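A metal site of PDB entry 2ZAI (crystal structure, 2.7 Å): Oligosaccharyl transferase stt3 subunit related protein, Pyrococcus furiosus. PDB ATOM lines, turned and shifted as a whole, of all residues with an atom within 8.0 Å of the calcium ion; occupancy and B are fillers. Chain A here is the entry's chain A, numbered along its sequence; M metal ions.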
ATOM      1  N   GLY A  80      19.629 -26.827  -6.745  1.00  0.00           N
ATOM      2  CA  GLY A  80      18.889 -25.636  -7.110  1.00  0.00           C
ATOM      3  C   GLY A  80      19.753 -24.491  -7.636  1.00  0.00           C
ATOM      4  O   GLY A  80      20.939 -24.663  -7.938  1.00  0.00           O
ATOM      5  N   ASN A  81      19.155 -23.311  -7.724  1.00  0.00           N
ATOM      6  CA  ASN A  81      19.831 -22.137  -8.276  1.00  0.00           C
ATOM      7  C   ASN A  81      21.251 -21.906  -7.871  1.00  0.00           C
ATOM      8  O   ASN A  81      22.111 -21.660  -8.724  1.00  0.00           O
ATOM      9  CB  ASN A  81      19.021 -20.885  -7.953  1.00  0.00           C
ATOM     10  CG  ASN A  81      17.740 -20.824  -8.713  1.00  0.00           C
ATOM     11  OD1 ASN A  81      17.352 -21.804  -9.349  1.00  0.00           O
ATOM     12  ND2 ASN A  81      17.057 -19.689  -8.650  1.00  0.00           N
ATOM     13  N   GLU A  84      24.278 -23.723  -9.374  1.00  0.00           N
ATOM     14  CA  GLU A  84      24.634 -23.468 -10.762  1.00  0.00           C
ATOM     15  C   GLU A  84      25.858 -22.555 -10.896  1.00  0.00           C
ATOM     16  O   GLU A  84      25.765 -21.331 -10.864  1.00  0.00           O
ATOM     17  CB  GLU A  84      23.428 -22.941 -11.519  1.00  0.00           C
ATOM     18  CG  GLU A  84      22.524 -24.096 -11.947  1.00  0.00           C
ATOM     19  CD  GLU A  84      21.432 -23.678 -12.892  1.00  0.00           C
ATOM     20  OE1 GLU A  84      21.746 -22.998 -13.905  1.00  0.00           O
ATOM     21  OE2 GLU A  84      20.256 -24.014 -12.645  1.00  0.00           O
ATOM     22  N   PHE A 232      14.797 -29.385 -12.255  1.00  0.00           N
ATOM     23  CA  PHE A 232      16.233 -29.184 -12.087  1.00  0.00           C
ATOM     24  C   PHE A 232      17.031 -30.412 -12.493  1.00  0.00           C
ATOM     25  O   PHE A 232      17.988 -30.316 -13.247  1.00  0.00           O
ATOM     26  CB  PHE A 232      16.578 -28.836 -10.632  1.00  0.00           C
ATOM     27  CG  PHE A 232      18.032 -28.494 -10.415  1.00  0.00           C
ATOM     28  CD1 PHE A 232      18.490 -27.173 -10.577  1.00  0.00           C
ATOM     29  CD2 PHE A 232      18.960 -29.487 -10.087  1.00  0.00           C
ATOM     30  CE1 PHE A 232      19.848 -26.854 -10.412  1.00  0.00           C
ATOM     31  CE2 PHE A 232      20.313 -29.172  -9.930  1.00  0.00           C
ATOM     32  CZ  PHE A 232      20.760 -27.860 -10.093  1.00  0.00           C
ATOM     33  N   LYS A 235      17.133 -31.108 -16.189  1.00  0.00           N
ATOM     34  CA  LYS A 235      18.033 -30.134 -16.788  1.00  0.00           C
ATOM     35  C   LYS A 235      19.496 -30.455 -16.521  1.00  0.00           C
ATOM     36  O   LYS A 235      20.321 -30.427 -17.438  1.00  0.00           O
ATOM     37  CB  LYS A 235      17.725 -28.730 -16.278  1.00  0.00           C
ATOM     38  CG  LYS A 235      16.377 -28.220 -16.711  1.00  0.00           C
ATOM     39  CD  LYS A 235      16.088 -26.857 -16.141  1.00  0.00           C
ATOM     40  CE  LYS A 235      14.805 -26.344 -16.729  1.00  0.00           C
ATOM     41  NZ  LYS A 235      14.324 -25.141 -16.019  1.00  0.00           N
ATOM     42  N   LEU A 236      19.823 -30.755 -15.270  1.00  0.00           N
ATOM     43  CA  LEU A 236      21.212 -31.042 -14.900  1.00  0.00           C
ATOM     44  C   LEU A 236      21.837 -32.124 -15.776  1.00  0.00           C
ATOM     45  O   LEU A 236      23.003 -32.015 -16.193  1.00  0.00           O
ATOM     46  CB  LEU A 236      21.332 -31.469 -13.435  1.00  0.00           C
ATOM     47  CG  LEU A 236      22.779 -31.692 -12.953  1.00  0.00           C
ATOM     48  CD1 LEU A 236      23.381 -30.370 -12.539  1.00  0.00           C
ATOM     49  CD2 LEU A 236      22.796 -32.634 -11.779  1.00  0.00           C
ATOM     50  N   ASN A 239      23.181 -31.237 -19.066  1.00  0.00           N
ATOM     51  CA  ASN A 239      24.425 -30.476 -18.923  1.00  0.00           C
ATOM     52  C   ASN A 239      25.615 -31.345 -18.568  1.00  0.00           C
ATOM     53  O   ASN A 239      26.755 -30.983 -18.855  1.00  0.00           O
ATOM     54  CB  ASN A 239      24.246 -29.421 -17.850  1.00  0.00           C
ATOM     55  CG  ASN A 239      23.256 -28.368 -18.257  1.00  0.00           C
ATOM     56  OD1 ASN A 239      23.550 -27.523 -19.112  1.00  0.00           O
ATOM     57  ND2 ASN A 239      22.071 -28.404 -17.662  1.00  0.00           N
ATOM     58  N   PRO A 256      27.580 -26.190 -20.835  1.00  0.00           N
ATOM     59  CA  PRO A 256      26.787 -25.136 -20.183  1.00  0.00           C
ATOM     60  C   PRO A 256      25.400 -25.006 -20.809  1.00  0.00           C
ATOM     61  O   PRO A 256      24.498 -24.417 -20.202  1.00  0.00           O
ATOM     62  CB  PRO A 256      27.627 -23.885 -20.386  1.00  0.00           C
ATOM     63  CG  PRO A 256      28.394 -24.186 -21.654  1.00  0.00           C
ATOM     64  CD  PRO A 256      28.773 -25.631 -21.500  1.00  0.00           C
ATOM     65  N   ILE A 287      15.597 -26.136 -23.426  1.00  0.00           N
ATOM     66  CA  ILE A 287      17.008 -25.914 -23.157  1.00  0.00           C
ATOM     67  C   ILE A 287      17.356 -25.694 -21.692  1.00  0.00           C
ATOM     68  O   ILE A 287      16.631 -25.021 -20.963  1.00  0.00           O
ATOM     69  CB  ILE A 287      17.510 -24.694 -23.940  1.00  0.00           C
ATOM     70  CG1 ILE A 287      17.386 -24.971 -25.444  1.00  0.00           C
ATOM     71  CG2 ILE A 287      18.925 -24.338 -23.516  1.00  0.00           C
ATOM     72  CD1 ILE A 287      17.889 -23.831 -26.334  1.00  0.00           C
ATOM     73  N   SER A 288      18.477 -26.262 -21.266  1.00  0.00           N
ATOM     74  CA  SER A 288      18.968 -26.070 -19.917  1.00  0.00           C
ATOM     75  C   SER A 288      20.252 -25.264 -20.040  1.00  0.00           C
ATOM     76  O   SER A 288      21.188 -25.672 -20.749  1.00  0.00           O
ATOM     77  CB  SER A 288      19.286 -27.405 -19.241  1.00  0.00           C
ATOM     78  OG  SER A 288      19.823 -27.196 -17.947  1.00  0.00           O
ATOM     79  N   ALA A 289      20.295 -24.100 -19.409  1.00  0.00           N
ATOM     80  CA  ALA A 289      21.483 -23.266 -19.437  1.00  0.00           C
ATOM     81  C   ALA A 289      22.104 -23.347 -18.043  1.00  0.00           C
ATOM     82  O   ALA A 289      21.525 -22.891 -17.043  1.00  0.00           O
ATOM     83  CB  ALA A 289      21.125 -21.838 -19.771  1.00  0.00           C
ATOM     84  N   PHE A 290      23.299 -23.926 -17.958  1.00  0.00           N
ATOM     85  CA  PHE A 290      23.955 -24.074 -16.662  1.00  0.00           C
ATOM     86  C   PHE A 290      25.078 -23.118 -16.345  1.00  0.00           C
ATOM     87  O   PHE A 290      26.162 -23.192 -16.930  1.00  0.00           O
ATOM     88  CB  PHE A 290      24.473 -25.508 -16.521  1.00  0.00           C
ATOM     89  CG  PHE A 290      24.691 -25.927 -15.104  1.00  0.00           C
ATOM     90  CD1 PHE A 290      23.668 -26.530 -14.392  1.00  0.00           C
ATOM     91  CD2 PHE A 290      25.930 -25.722 -14.489  1.00  0.00           C
ATOM     92  CE1 PHE A 290      23.869 -26.943 -13.060  1.00  0.00           C
ATOM     93  CE2 PHE A 290      26.154 -26.127 -13.177  1.00  0.00           C
ATOM     94  CZ  PHE A 290      25.115 -26.745 -12.446  1.00  0.00           C
ATOM     95  N   GLY A 291      24.830 -22.198 -15.406  1.00  0.00           N
ATOM     96  CA  GLY A 291      25.867 -21.271 -14.985  1.00  0.00           C
ATOM     97  C   GLY A 291      25.953 -19.935 -15.674  1.00  0.00           C
ATOM     98  O   GLY A 291      26.429 -18.968 -15.081  1.00  0.00           O
ATOM     99  N   ARG A 292      25.534 -19.868 -16.926  1.00  0.00           N
ATOM    100  CA  ARG A 292      25.581 -18.602 -17.657  1.00  0.00           C
ATOM    101  C   ARG A 292      24.428 -18.454 -18.621  1.00  0.00           C
ATOM    102  O   ARG A 292      23.735 -19.417 -18.951  1.00  0.00           O
ATOM    103  CB  ARG A 292      26.906 -18.473 -18.413  1.00  0.00           C
ATOM    104  CG  ARG A 292      27.206 -19.624 -19.339  1.00  0.00           C
ATOM    105  CD  ARG A 292      28.488 -19.384 -20.134  1.00  0.00           C
ATOM    106  NE  ARG A 292      29.531 -18.829 -19.302  1.00  0.00           N
ATOM    107  CZ  ARG A 292      30.633 -18.247 -19.767  1.00  0.00           C
ATOM    108  NH1 ARG A 292      30.839 -18.165 -21.065  1.00  0.00           N
ATOM    109  NH2 ARG A 292      31.530 -17.750 -18.920  1.00  0.00           N
ATOM    110  N   ASP A 322      17.803 -16.356 -19.678  1.00  0.00           N
ATOM    111  CA  ASP A 322      18.318 -16.327 -18.316  1.00  0.00           C
ATOM    112  C   ASP A 322      18.686 -17.742 -17.889  1.00  0.00           C
ATOM    113  O   ASP A 322      17.870 -18.654 -18.037  1.00  0.00           O
ATOM    114  CB  ASP A 322      17.273 -15.757 -17.371  1.00  0.00           C
ATOM    115  CG  ASP A 322      17.727 -15.773 -15.942  1.00  0.00           C
ATOM    116  OD1 ASP A 322      18.907 -15.414 -15.697  1.00  0.00           O
ATOM    117  OD2 ASP A 322      16.910 -16.129 -15.064  1.00  0.00           O
ATOM    118  N   TYR A 323      19.886 -17.928 -17.355  1.00  0.00           N
ATOM    119  CA  TYR A 323      20.318 -19.263 -16.934  1.00  0.00           C
ATOM    120  C   TYR A 323      19.552 -19.818 -15.712  1.00  0.00           C
ATOM    121  O   TYR A 323      19.706 -20.985 -15.376  1.00  0.00           O
ATOM    122  CB  TYR A 323      21.841 -19.294 -16.724  1.00  0.00           C
ATOM    123  CG  TYR A 323      22.356 -18.725 -15.424  1.00  0.00           C
ATOM    124  CD1 TYR A 323      22.281 -19.445 -14.243  1.00  0.00           C
ATOM    125  CD2 TYR A 323      22.908 -17.450 -15.377  1.00  0.00           C
ATOM    126  CE1 TYR A 323      22.743 -18.924 -13.040  1.00  0.00           C
ATOM    127  CE2 TYR A 323      23.374 -16.911 -14.187  1.00  0.00           C
ATOM    128  CZ  TYR A 323      23.282 -17.643 -13.014  1.00  0.00           C
ATOM    129  OH  TYR A 323      23.685 -17.106 -11.817  1.00  0.00           O
ATOM    130  N   LEU A 324      18.741 -18.987 -15.068  1.00  0.00           N
ATOM    131  CA  LEU A 324      17.950 -19.426 -13.913  1.00  0.00           C
ATOM    132  C   LEU A 324      16.461 -19.445 -14.255  1.00  0.00           C
ATOM    133  O   LEU A 324      15.627 -19.799 -13.419  1.00  0.00           O
ATOM    134  CB  LEU A 324      18.181 -18.538 -12.690  1.00  0.00           C
ATOM    135  CG  LEU A 324      19.524 -18.636 -11.969  1.00  0.00           C
ATOM    136  CD1 LEU A 324      19.432 -17.937 -10.616  1.00  0.00           C
ATOM    137  CD2 LEU A 324      19.904 -20.098 -11.766  1.00  0.00           C
ATOM    138  N   ASN A 325      16.134 -19.057 -15.484  1.00  0.00           N
ATOM    139  CA  ASN A 325      14.752 -19.017 -15.933  1.00  0.00           C
ATOM    140  C   ASN A 325      14.599 -19.293 -17.417  1.00  0.00           C
ATOM    141  O   ASN A 325      14.224 -18.424 -18.202  1.00  0.00           O
ATOM    142  CB  ASN A 325      14.114 -17.675 -15.594  1.00  0.00           C
ATOM    143  CG  ASN A 325      13.058 -17.805 -14.525  1.00  0.00           C
ATOM    144  OD1 ASN A 325      12.079 -18.552 -14.679  1.00  0.00           O
ATOM    145  ND2 ASN A 325      13.239 -17.079 -13.410  1.00  0.00           N
ATOM    146  N   GLU A 326      14.883 -20.534 -17.805  1.00  0.00           N
ATOM    147  CA  GLU A 326      14.785 -20.943 -19.194  1.00  0.00           C
ATOM    148  C   GLU A 326      13.356 -20.953 -19.678  1.00  0.00           C
ATOM    149  O   GLU A 326      12.426 -20.952 -18.886  1.00  0.00           O
ATOM    150  CB  GLU A 326      15.396 -22.335 -19.382  1.00  0.00           C
ATOM    151  CG  GLU A 326      16.900 -22.419 -19.185  1.00  0.00           C
ATOM    152  CD  GLU A 326      17.350 -22.841 -17.774  1.00  0.00           C
ATOM    153  OE1 GLU A 326      18.551 -23.133 -17.626  1.00  0.00           O
ATOM    154  OE2 GLU A 326      16.514 -22.879 -16.844  1.00  0.00           O
HETATM  155 CA    CA M   1      19.646 -23.508 -15.278  1.00  0.00          CA
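The side-chain carboxylate (OE2) of Glu 326 lies within salt-bridge range of the side-chain amino group (NZ) of Lys 235, 3.3 Å away.
Of the 19 residues printed, 4 come within 4 Å of the calcium ion.
O of Tyr 323 binds the calcium ion (2.5 Å). OE1 of Glu 84 binds the calcium ion. The calcium ion is bound by the side-chain carboxylate (OE1) of Glu 326, 2.6 Å away. O of Ala 289 is bound to the calcium ion (2.7 Å). OE2 of Glu 84 binds the calcium ion, 2.7 Å away.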
